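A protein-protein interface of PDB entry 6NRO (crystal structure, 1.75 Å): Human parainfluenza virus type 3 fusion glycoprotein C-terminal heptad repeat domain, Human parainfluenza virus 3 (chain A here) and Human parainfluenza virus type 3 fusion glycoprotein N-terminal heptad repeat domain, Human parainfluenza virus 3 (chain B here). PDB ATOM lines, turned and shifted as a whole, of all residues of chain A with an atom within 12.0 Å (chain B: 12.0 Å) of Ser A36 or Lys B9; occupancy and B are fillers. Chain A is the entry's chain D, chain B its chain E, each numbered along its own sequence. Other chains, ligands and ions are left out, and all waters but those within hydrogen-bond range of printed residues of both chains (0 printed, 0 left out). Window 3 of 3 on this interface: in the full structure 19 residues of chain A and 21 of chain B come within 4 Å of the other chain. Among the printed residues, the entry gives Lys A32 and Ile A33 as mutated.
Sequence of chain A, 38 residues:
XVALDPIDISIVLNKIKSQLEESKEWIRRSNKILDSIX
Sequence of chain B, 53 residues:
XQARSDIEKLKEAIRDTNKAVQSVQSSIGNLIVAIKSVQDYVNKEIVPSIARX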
ATOM      1  N   TRP A  26     -22.644 -12.781   9.888  1.00  0.00           N
ATOM      2  CA  TRP A  26     -22.855 -11.780   8.841  1.00  0.00           C
ATOM      3  C   TRP A  26     -24.170 -12.014   8.109  1.00  0.00           C
ATOM      4  O   TRP A  26     -24.874 -11.056   7.755  1.00  0.00           O
ATOM      5  CB  TRP A  26     -21.698 -11.787   7.839  1.00  0.00           C
ATOM      6  CG  TRP A  26     -20.437 -11.150   8.357  1.00  0.00           C
ATOM      7  CD1 TRP A  26     -19.191 -11.712   8.428  1.00  0.00           C
ATOM      8  CD2 TRP A  26     -20.308  -9.828   8.890  1.00  0.00           C
ATOM      9  NE1 TRP A  26     -18.298 -10.819   8.966  1.00  0.00           N
ATOM     10  CE2 TRP A  26     -18.961  -9.655   9.263  1.00  0.00           C
ATOM     11  CE3 TRP A  26     -21.203  -8.769   9.088  1.00  0.00           C
ATOM     12  CZ2 TRP A  26     -18.485  -8.467   9.829  1.00  0.00           C
ATOM     13  CZ3 TRP A  26     -20.732  -7.587   9.639  1.00  0.00           C
ATOM     14  CH2 TRP A  26     -19.383  -7.446   9.999  1.00  0.00           C
ATOM     15  N   ILE A  27     -24.518 -13.256   7.834  1.00  0.00           N
ATOM     16  CA  ILE A  27     -25.758 -13.537   7.155  1.00  0.00           C
ATOM     17  C   ILE A  27     -26.904 -13.171   8.081  1.00  0.00           C
ATOM     18  O   ILE A  27     -27.881 -12.631   7.653  1.00  0.00           O
ATOM     19  CB  ILE A  27     -25.847 -14.994   6.705  1.00  0.00           C
ATOM     20  CG1 ILE A  27     -24.910 -15.226   5.533  1.00  0.00           C
ATOM     21  CG2 ILE A  27     -27.263 -15.365   6.335  1.00  0.00           C
ATOM     22  CD1 ILE A  27     -25.184 -14.364   4.345  1.00  0.00           C
ATOM     23  N   ARG A  28     -26.755 -13.414   9.378  1.00  0.00           N
ATOM     24  CA  ARG A  28     -27.791 -13.035  10.330  1.00  0.00           C
ATOM     25  C   ARG A  28     -27.968 -11.542  10.310  1.00  0.00           C
ATOM     26  O   ARG A  28     -29.073 -11.063  10.340  1.00  0.00           O
ATOM     27  CB  ARG A  28     -27.480 -13.461  11.763  1.00  0.00           C
ATOM     28  CG  ARG A  28     -28.714 -13.442  12.675  1.00  0.00           C
ATOM     29  CD  ARG A  28     -28.447 -13.316  14.171  1.00  0.00           C
ATOM     30  NE  ARG A  28     -27.563 -12.210  14.493  1.00  0.00           N
ATOM     31  CZ  ARG A  28     -27.949 -10.969  14.753  1.00  0.00           C
ATOM     32  NH1 ARG A  28     -29.230 -10.639  14.747  1.00  0.00           N
ATOM     33  NH2 ARG A  28     -27.040 -10.054  15.021  1.00  0.00           N
ATOM     34  N   ARG A  29     -26.883 -10.799  10.272  1.00  0.00           N
ATOM     35  CA  ARG A  29     -26.987  -9.372  10.201  1.00  0.00           C
ATOM     36  C   ARG A  29     -27.618  -8.900   8.898  1.00  0.00           C
ATOM     37  O   ARG A  29     -28.410  -7.996   8.912  1.00  0.00           O
ATOM     38  CB  ARG A  29     -25.630  -8.763  10.376  1.00  0.00           C
ATOM     39  CG  ARG A  29     -25.093  -9.009  11.762  1.00  0.00           C
ATOM     40  CD  ARG A  29     -23.774  -8.322  11.991  1.00  0.00           C
ATOM     41  NE  ARG A  29     -23.430  -8.419  13.388  1.00  0.00           N
ATOM     42  CZ  ARG A  29     -22.467  -7.735  13.953  1.00  0.00           C
ATOM     43  NH1 ARG A  29     -21.737  -6.885  13.261  1.00  0.00           N
ATOM     44  NH2 ARG A  29     -22.241  -7.915  15.231  1.00  0.00           N
ATOM     45  N   SER A  30     -27.250  -9.508   7.781  1.00  0.00           N
ATOM     46  CA  SER A  30     -27.854  -9.132   6.509  1.00  0.00           C
ATOM     47  C   SER A  30     -29.363  -9.315   6.558  1.00  0.00           C
ATOM     48  O   SER A  30     -30.127  -8.409   6.206  1.00  0.00           O
ATOM     49  CB  SER A  30     -27.234  -9.959   5.388  1.00  0.00           C
ATOM     50  OG  SER A  30     -27.838  -9.685   4.140  1.00  0.00           O
ATOM     51  N   ASN A  31     -29.809 -10.483   7.021  1.00  0.00           N
ATOM     52  CA  ASN A  31     -31.238 -10.771   7.046  1.00  0.00           C
ATOM     53  C   ASN A  31     -31.979  -9.837   7.998  1.00  0.00           C
ATOM     54  O   ASN A  31     -33.109  -9.424   7.714  1.00  0.00           O
ATOM     55  CB  ASN A  31     -31.454 -12.228   7.429  1.00  0.00           C
ATOM     56  CG  ASN A  31     -31.102 -13.178   6.299  1.00  0.00           C
ATOM     57  OD1 ASN A  31     -31.295 -12.866   5.119  1.00  0.00           O
ATOM     58  ND2 ASN A  31     -30.593 -14.340   6.654  1.00  0.00           N
ATOM     59  N   LYS A  32     -31.351  -9.476   9.116  1.00  0.00           N
ATOM     60  CA  LYS A  32     -31.986  -8.540  10.038  1.00  0.00           C
ATOM     61  C   LYS A  32     -32.227  -7.190   9.370  1.00  0.00           C
ATOM     62  O   LYS A  32     -33.266  -6.554   9.593  1.00  0.00           O
ATOM     63  CB  LYS A  32     -31.128  -8.386  11.289  1.00  0.00           C
ATOM     64  CG  LYS A  32     -31.270  -9.537  12.246  1.00  0.00           C
ATOM     65  N   ILE A  33     -31.286  -6.736   8.541  1.00  0.00           N
ATOM     66  CA  ILE A  33     -31.479  -5.462   7.860  1.00  0.00           C
ATOM     67  C   ILE A  33     -32.607  -5.571   6.846  1.00  0.00           C
ATOM     68  O   ILE A  33     -33.477  -4.698   6.766  1.00  0.00           O
ATOM     69  CB  ILE A  33     -30.178  -4.986   7.187  1.00  0.00           C
ATOM     70  CG1 ILE A  33     -29.127  -4.669   8.253  1.00  0.00           C
ATOM     71  CG2 ILE A  33     -30.449  -3.756   6.347  1.00  0.00           C
ATOM     72  CD1 ILE A  33     -27.729  -4.378   7.715  1.00  0.00           C
ATOM     73  N   LEU A  34     -32.622  -6.666   6.090  1.00  0.00           N
ATOM     74  CA  LEU A  34     -33.644  -6.917   5.050  1.00  0.00           C
ATOM     75  C   LEU A  34     -35.019  -6.935   5.718  1.00  0.00           C
ATOM     76  O   LEU A  34     -35.958  -6.474   5.110  1.00  0.00           O
ATOM     77  CB  LEU A  34     -33.370  -8.235   4.314  1.00  0.00           C
ATOM     78  CG  LEU A  34     -32.054  -8.330   3.550  1.00  0.00           C
ATOM     79  CD1 LEU A  34     -31.900  -9.702   2.929  1.00  0.00           C
ATOM     80  CD2 LEU A  34     -31.925  -7.266   2.484  1.00  0.00           C
ATOM     81  N   ASP A  35     -35.110  -7.446   6.941  1.00  0.00           N
ATOM     82  CA  ASP A  35     -36.378  -7.522   7.706  1.00  0.00           C
ATOM     83  C   ASP A  35     -36.908  -6.108   7.978  1.00  0.00           C
ATOM     84  O   ASP A  35     -38.121  -5.942   8.052  1.00  0.00           O
ATOM     85  CB  ASP A  35     -36.168  -8.255   9.025  1.00  0.00           C
ATOM     86  CG  ASP A  35     -36.067  -9.754   8.892  1.00  0.00           C
ATOM     87  OD1 ASP A  35     -36.316 -10.260   7.808  1.00  0.00           O
ATOM     88  OD2 ASP A  35     -35.753 -10.383   9.889  1.00  0.00           O
ATOM     89  N   SER A  36     -36.018  -5.137   8.129  1.00  0.00           N
ATOM     90  CA  SER A  36     -36.358  -3.736   8.456  1.00  0.00           C
ATOM     91  C   SER A  36     -36.916  -3.019   7.222  1.00  0.00           C
ATOM     92  O   SER A  36     -37.441  -1.936   7.402  1.00  0.00           O
ATOM     93  CB  SER A  36     -35.180  -3.036   9.050  1.00  0.00           C
ATOM     94  OG  SER A  36     -34.285  -2.603   8.055  1.00  0.00           O
ATOM     95  N   ILE A  37     -36.804  -3.599   6.030  1.00  0.00           N
ATOM     96  CA  ILE A  37     -37.343  -3.032   4.764  1.00  0.00           C
ATOM     97  C   ILE A  37     -38.774  -3.538   4.611  1.00  0.00           C
ATOM     98  O   ILE A  37     -38.913  -4.568   3.958  1.00  0.00           O
ATOM     99  CB  ILE A  37     -36.477  -3.428   3.559  1.00  0.00           C
ATOM    100  CG1 ILE A  37     -35.058  -2.885   3.678  1.00  0.00           C
ATOM    101  CG2 ILE A  37     -37.124  -2.997   2.266  1.00  0.00           C
ATOM    102  CD1 ILE A  37     -34.130  -3.375   2.614  1.00  0.00           C
ATOM    103  N   ARG B   4     -33.121   5.390   8.298  1.00  0.00           N
ATOM    104  CA  ARG B   4     -32.322   5.034   7.098  1.00  0.00           C
ATOM    105  C   ARG B   4     -33.285   4.586   5.986  1.00  0.00           C
ATOM    106  O   ARG B   4     -34.315   3.998   6.315  1.00  0.00           O
ATOM    107  CB  ARG B   4     -31.273   3.989   7.490  1.00  0.00           C
ATOM    108  N   SER B   5     -32.966   4.857   4.718  1.00  0.00           N
ATOM    109  CA  SER B   5     -33.830   4.557   3.544  1.00  0.00           C
ATOM    110  C   SER B   5     -33.779   3.076   3.170  1.00  0.00           C
ATOM    111  O   SER B   5     -32.952   2.356   3.691  1.00  0.00           O
ATOM    112  CB  SER B   5     -33.462   5.419   2.361  1.00  0.00           C
ATOM    113  OG  SER B   5     -32.152   5.158   1.907  1.00  0.00           O
ATOM    114  N   ASP B   6     -34.670   2.658   2.283  1.00  0.00           N
ATOM    115  CA  ASP B   6     -34.739   1.273   1.771  1.00  0.00           C
ATOM    116  C   ASP B   6     -33.467   1.010   0.964  1.00  0.00           C
ATOM    117  O   ASP B   6     -32.904  -0.065   1.095  1.00  0.00           O
ATOM    118  CB  ASP B   6     -36.023   1.061   0.968  1.00  0.00           C
ATOM    119  CG  ASP B   6     -37.264   0.939   1.831  1.00  0.00           C
ATOM    120  OD1 ASP B   6     -37.120   0.921   3.050  1.00  0.00           O
ATOM    121  OD2 ASP B   6     -38.356   0.849   1.275  1.00  0.00           O
ATOM    122  N   ILE B   7     -33.007   1.972   0.179  1.00  0.00           N
ATOM    123  CA  ILE B   7     -31.783   1.813  -0.649  1.00  0.00           C
ATOM    124  C   ILE B   7     -30.579   1.627   0.269  1.00  0.00           C
ATOM    125  O   ILE B   7     -29.756   0.793  -0.039  1.00  0.00           O
ATOM    126  CB  ILE B   7     -31.560   3.011  -1.576  1.00  0.00           C
ATOM    127  CG1 ILE B   7     -32.606   3.080  -2.689  1.00  0.00           C
ATOM    128  CG2 ILE B   7     -30.144   3.006  -2.115  1.00  0.00           C
ATOM    129  CD1 ILE B   7     -32.583   1.920  -3.625  1.00  0.00           C
ATOM    130  N   GLU B   8     -30.477   2.408   1.340  1.00  0.00           N
ATOM    131  CA  GLU B   8     -29.323   2.343   2.264  1.00  0.00           C
ATOM    132  C   GLU B   8     -29.342   0.975   2.937  1.00  0.00           C
ATOM    133  O   GLU B   8     -28.309   0.339   3.015  1.00  0.00           O
ATOM    134  CB  GLU B   8     -29.364   3.489   3.269  1.00  0.00           C
ATOM    135  N   LYS B   9     -30.508   0.551   3.390  1.00  0.00           N
ATOM    136  CA  LYS B   9     -30.670  -0.764   4.020  1.00  0.00           C
ATOM    137  C   LYS B   9     -30.188  -1.835   3.031  1.00  0.00           C
ATOM    138  O   LYS B   9     -29.397  -2.645   3.435  1.00  0.00           O
ATOM    139  CB  LYS B   9     -32.116  -0.958   4.463  1.00  0.00           C
ATOM    140  CG  LYS B   9     -32.578  -0.034   5.581  1.00  0.00           C
ATOM    141  CD  LYS B   9     -34.064  -0.116   5.824  1.00  0.00           C
ATOM    142  CE  LYS B   9     -34.487   0.260   7.224  1.00  0.00           C
ATOM    143  NZ  LYS B   9     -35.954   0.387   7.322  1.00  0.00           N
ATOM    144  N   LEU B  10     -30.585  -1.802   1.759  1.00  0.00           N
ATOM    145  CA  LEU B  10     -30.203  -2.840   0.802  1.00  0.00           C
ATOM    146  C   LEU B  10     -28.695  -2.852   0.566  1.00  0.00           C
ATOM    147  O   LEU B  10     -28.077  -3.920   0.508  1.00  0.00           O
ATOM    148  CB  LEU B  10     -30.940  -2.641  -0.516  1.00  0.00           C
ATOM    149  CG  LEU B  10     -32.435  -2.912  -0.518  1.00  0.00           C
ATOM    150  CD1 LEU B  10     -33.064  -2.383  -1.843  1.00  0.00           C
ATOM    151  CD2 LEU B  10     -32.714  -4.366  -0.351  1.00  0.00           C
ATOM    152  N   LYS B  11     -28.094  -1.684   0.480  1.00  0.00           N
ATOM    153  CA  LYS B  11     -26.634  -1.559   0.287  1.00  0.00           C
ATOM    154  C   LYS B  11     -25.905  -2.216   1.462  1.00  0.00           C
ATOM    155  O   LYS B  11     -24.958  -2.916   1.210  1.00  0.00           O
ATOM    156  CB  LYS B  11     -26.253  -0.084   0.170  1.00  0.00           C
ATOM    157  CG  LYS B  11     -24.779   0.193  -0.057  1.00  0.00           C
ATOM    158  CD  LYS B  11     -24.460   1.664  -0.096  1.00  0.00           C
ATOM    159  CE  LYS B  11     -23.262   2.039   0.742  1.00  0.00           C
ATOM    160  NZ  LYS B  11     -22.194   2.637  -0.088  1.00  0.00           N
ATOM    161  N   GLU B  12     -26.328  -1.981   2.699  1.00  0.00           N
ATOM    162  CA  GLU B  12     -25.633  -2.558   3.879  1.00  0.00           C
ATOM    163  C   GLU B  12     -25.866  -4.072   3.915  1.00  0.00           C
ATOM    164  O   GLU B  12     -24.925  -4.796   4.184  1.00  0.00           O
ATOM    165  CB  GLU B  12     -26.046  -1.883   5.183  1.00  0.00           C
ATOM    166  N   ALA B  13     -27.080  -4.517   3.635  1.00  0.00           N
ATOM    167  CA  ALA B  13     -27.439  -5.946   3.587  1.00  0.00           C
ATOM    168  C   ALA B  13     -26.451  -6.668   2.672  1.00  0.00           C
ATOM    169  O   ALA B  13     -25.918  -7.676   3.102  1.00  0.00           O
ATOM    170  CB  ALA B  13     -28.849  -6.095   3.101  1.00  0.00           C
ATOM    171  N   ILE B  14     -26.260  -6.164   1.466  1.00  0.00           N
ATOM    172  CA  ILE B  14     -25.353  -6.775   0.470  1.00  0.00           C
ATOM    173  C   ILE B  14     -23.929  -6.688   1.002  1.00  0.00           C
ATOM    174  O   ILE B  14     -23.153  -7.573   0.710  1.00  0.00           O
ATOM    175  CB  ILE B  14     -25.509  -6.111  -0.903  1.00  0.00           C
ATOM    176  CG1 ILE B  14     -26.963  -6.123  -1.361  1.00  0.00           C
ATOM    177  CG2 ILE B  14     -24.597  -6.752  -1.914  1.00  0.00           C
ATOM    178  CD1 ILE B  14     -27.232  -5.248  -2.541  1.00  0.00           C
ATOM    179  N   ARG B  15     -23.599  -5.663   1.774  1.00  0.00           N
ATOM    180  CA  ARG B  15     -22.217  -5.547   2.288  1.00  0.00           C
ATOM    181  C   ARG B  15     -21.984  -6.661   3.312  1.00  0.00           C
ATOM    182  O   ARG B  15     -20.940  -7.245   3.266  1.00  0.00           O
ATOM    183  CB  ARG B  15     -21.911  -4.124   2.755  1.00  0.00           C
ATOM    184  CG  ARG B  15     -21.536  -3.221   1.586  1.00  0.00           C
ATOM    185  CD  ARG B  15     -20.594  -2.080   1.890  1.00  0.00           C
ATOM    186  NE  ARG B  15     -20.974  -1.371   3.092  1.00  0.00           N
ATOM    187  CZ  ARG B  15     -21.425  -0.129   3.121  1.00  0.00           C
ATOM    188  NH1 ARG B  15     -20.828   0.803   2.400  1.00  0.00           N
ATOM    189  NH2 ARG B  15     -22.465   0.175   3.878  1.00  0.00           N
ATOM    190  N   ASP B  16     -22.954  -6.972   4.151  1.00  0.00           N
ATOM    191  CA  ASP B  16     -22.818  -8.047   5.155  1.00  0.00           C
ATOM    192  C   ASP B  16     -22.742  -9.380   4.412  1.00  0.00           C
ATOM    193  O   ASP B  16     -21.928 -10.215   4.760  1.00  0.00           O
ATOM    194  CB  ASP B  16     -23.952  -7.993   6.165  1.00  0.00           C
ATOM    195  CG  ASP B  16     -23.807  -6.809   7.089  1.00  0.00           C
ATOM    196  OD1 ASP B  16     -24.748  -6.508   7.796  1.00  0.00           O
ATOM    197  OD2 ASP B  16     -22.755  -6.220   7.062  1.00  0.00           O
ATOM    198  N   THR B  17     -23.555  -9.562   3.390  1.00  0.00           N
ATOM    199  CA  THR B  17     -23.521 -10.803   2.632  1.00  0.00           C
ATOM    200  C   THR B  17     -22.155 -11.025   1.991  1.00  0.00           C
ATOM    201  O   THR B  17     -21.644 -12.148   1.973  1.00  0.00           O
ATOM    202  CB  THR B  17     -24.619 -10.789   1.579  1.00  0.00           C
ATOM    203  OG1 THR B  17     -25.892 -10.702   2.230  1.00  0.00           O
ATOM    204  CG2 THR B  17     -24.568 -12.038   0.719  1.00  0.00           C
ATOM    205  N   ASN B  18     -21.538  -9.971   1.470  1.00  0.00           N
ATOM    206  CA  ASN B  18     -20.208 -10.133   0.891  1.00  0.00           C
ATOM    207  C   ASN B  18     -19.192 -10.517   1.960  1.00  0.00           C
ATOM    208  O   ASN B  18     -18.307 -11.346   1.722  1.00  0.00           O
ATOM    209  CB  ASN B  18     -19.807  -8.845   0.167  1.00  0.00           C
ATOM    210  CG  ASN B  18     -20.630  -8.610  -1.113  1.00  0.00           C
ATOM    211  OD1 ASN B  18     -21.254  -9.530  -1.641  1.00  0.00           O
ATOM    212  ND2 ASN B  18     -20.612  -7.381  -1.611  1.00  0.00           N
ATOM    213  N   LYS B  19     -19.299  -9.922   3.146  1.00  0.00           N
ATOM    214  CA  LYS B  19     -18.409 -10.310   4.231  1.00  0.00           C
ATOM    215  C   LYS B  19     -18.620 -11.774   4.588  1.00  0.00           C
ATOM    216  O   LYS B  19     -17.657 -12.501   4.875  1.00  0.00           O
ATOM    217  CB  LYS B  19     -18.643  -9.401   5.438  1.00  0.00           C
ATOM    218  CG  LYS B  19     -18.188  -7.953   5.210  1.00  0.00           C
ATOM    219  CD  LYS B  19     -18.481  -7.080   6.422  1.00  0.00           C
ATOM    220  CE  LYS B  19     -17.790  -5.717   6.315  1.00  0.00           C
ATOM    221  NZ  LYS B  19     -18.721  -4.604   6.018  1.00  0.00           N
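O of Ser A36 is in hydrogen-bond range of NZ of Lys B9, 2.8 Å away.
The backbone carbonyl oxygen of Ala B13 sits at hydrogen-bond distance from the side-chain hydroxyl of Ser A30.
OG of Ser A30 lies within hydrogen-bond range of OG1 of Thr B17 (2.9 Å).
OG1 of Thr B17 sits at hydrogen-bond distance from O of Ala B13 (3.1 Å).
O of Ile A33 is in hydrogen-bond range of OG of Ser A36 (2.6 Å).
Among the printed residues, pairs that only touch across the chains: Ile A33 with Lys B9, Leu A34 with Ala B13, Ile A37 with Leu B10, Trp A26 with Asp B16, Arg A29 with Asp B16, Ile A37 with Lys B9, Ile A33 with Asp B16, Trp A26 with Lys B19, Ile A37 with Asp B6, Ser A30 with Asp B16 and Ile A33 with Glu B12.
Of the printed residues of chain B, Arg A29 touches Asp B16 (3.5 Å).
Of the printed residues of chain B, Ser A30 touches Ala B13 (3.0 Å), Asp B16 (3.9 Å) and Thr B17 (2.9 Å).
No residue of chain B comes within 4 Å of Lys A32.
Ile A33 touches just these residues of chain B: Lys B9, Glu B12 and Asp B16.
Of chain B, only Ala B13 (3.3 Å) comes within 4 Å of Leu A34.
No residue of chain B comes within 4 Å of Asp A35.
Ser A36 touches just one residue of chain B: Lys B9 (2.8 Å).
Ile A37 touches three residues of chain B.
No residue of chain A comes within 4 Å of Arg B4.
No residue of chain A comes within 4 Å of Ser B5.
Asp B6 touches just one residue of chain A: Ile A37.
No residue of chain A comes within 4 Å of Ile B7.
No residue of chain A comes within 4 Å of Glu B8.
Lys B9 touches just these residues of chain A: Ile A33, Ser A36 and Ile A37.
Lys B11 touches none of the printed residues of chain A.
Ala B13 touches two residues of chain A.
Of the printed residues of chain A, Asp B16 touches Trp A26 (3.5 Å), Arg A29 (3.5 Å), Ser A30 (3.9 Å) and Ile A33 (3.7 Å).
Printed residues of chain A within 4 Å of Thr B17: Ser A30.
Of the printed residues of chain A, Lys B19 touches Trp A26.
The nearest printed residue of chain A that does not touch Asp B16 is Ile A27 (5.0 Å).
Of the 16 printed residues of chain B, 8 touch a printed residue of chain A.
Hydrophobic or aromatic side chains of chain B that line the printed part of chain A: Leu B10 and Ala B13.
Of the 12 printed residues of chain A, 7 touch a printed residue of chain B.
Hydrophobic or aromatic side chains of chain A that line the printed part of chain B: Trp A26, Ile A33, Leu A34 and Ile A37.
Among the printed residues, no Asp or Glu carboxylate lies within 4 Å of a Lys or Arg side-chain nitrogen of the other chain.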
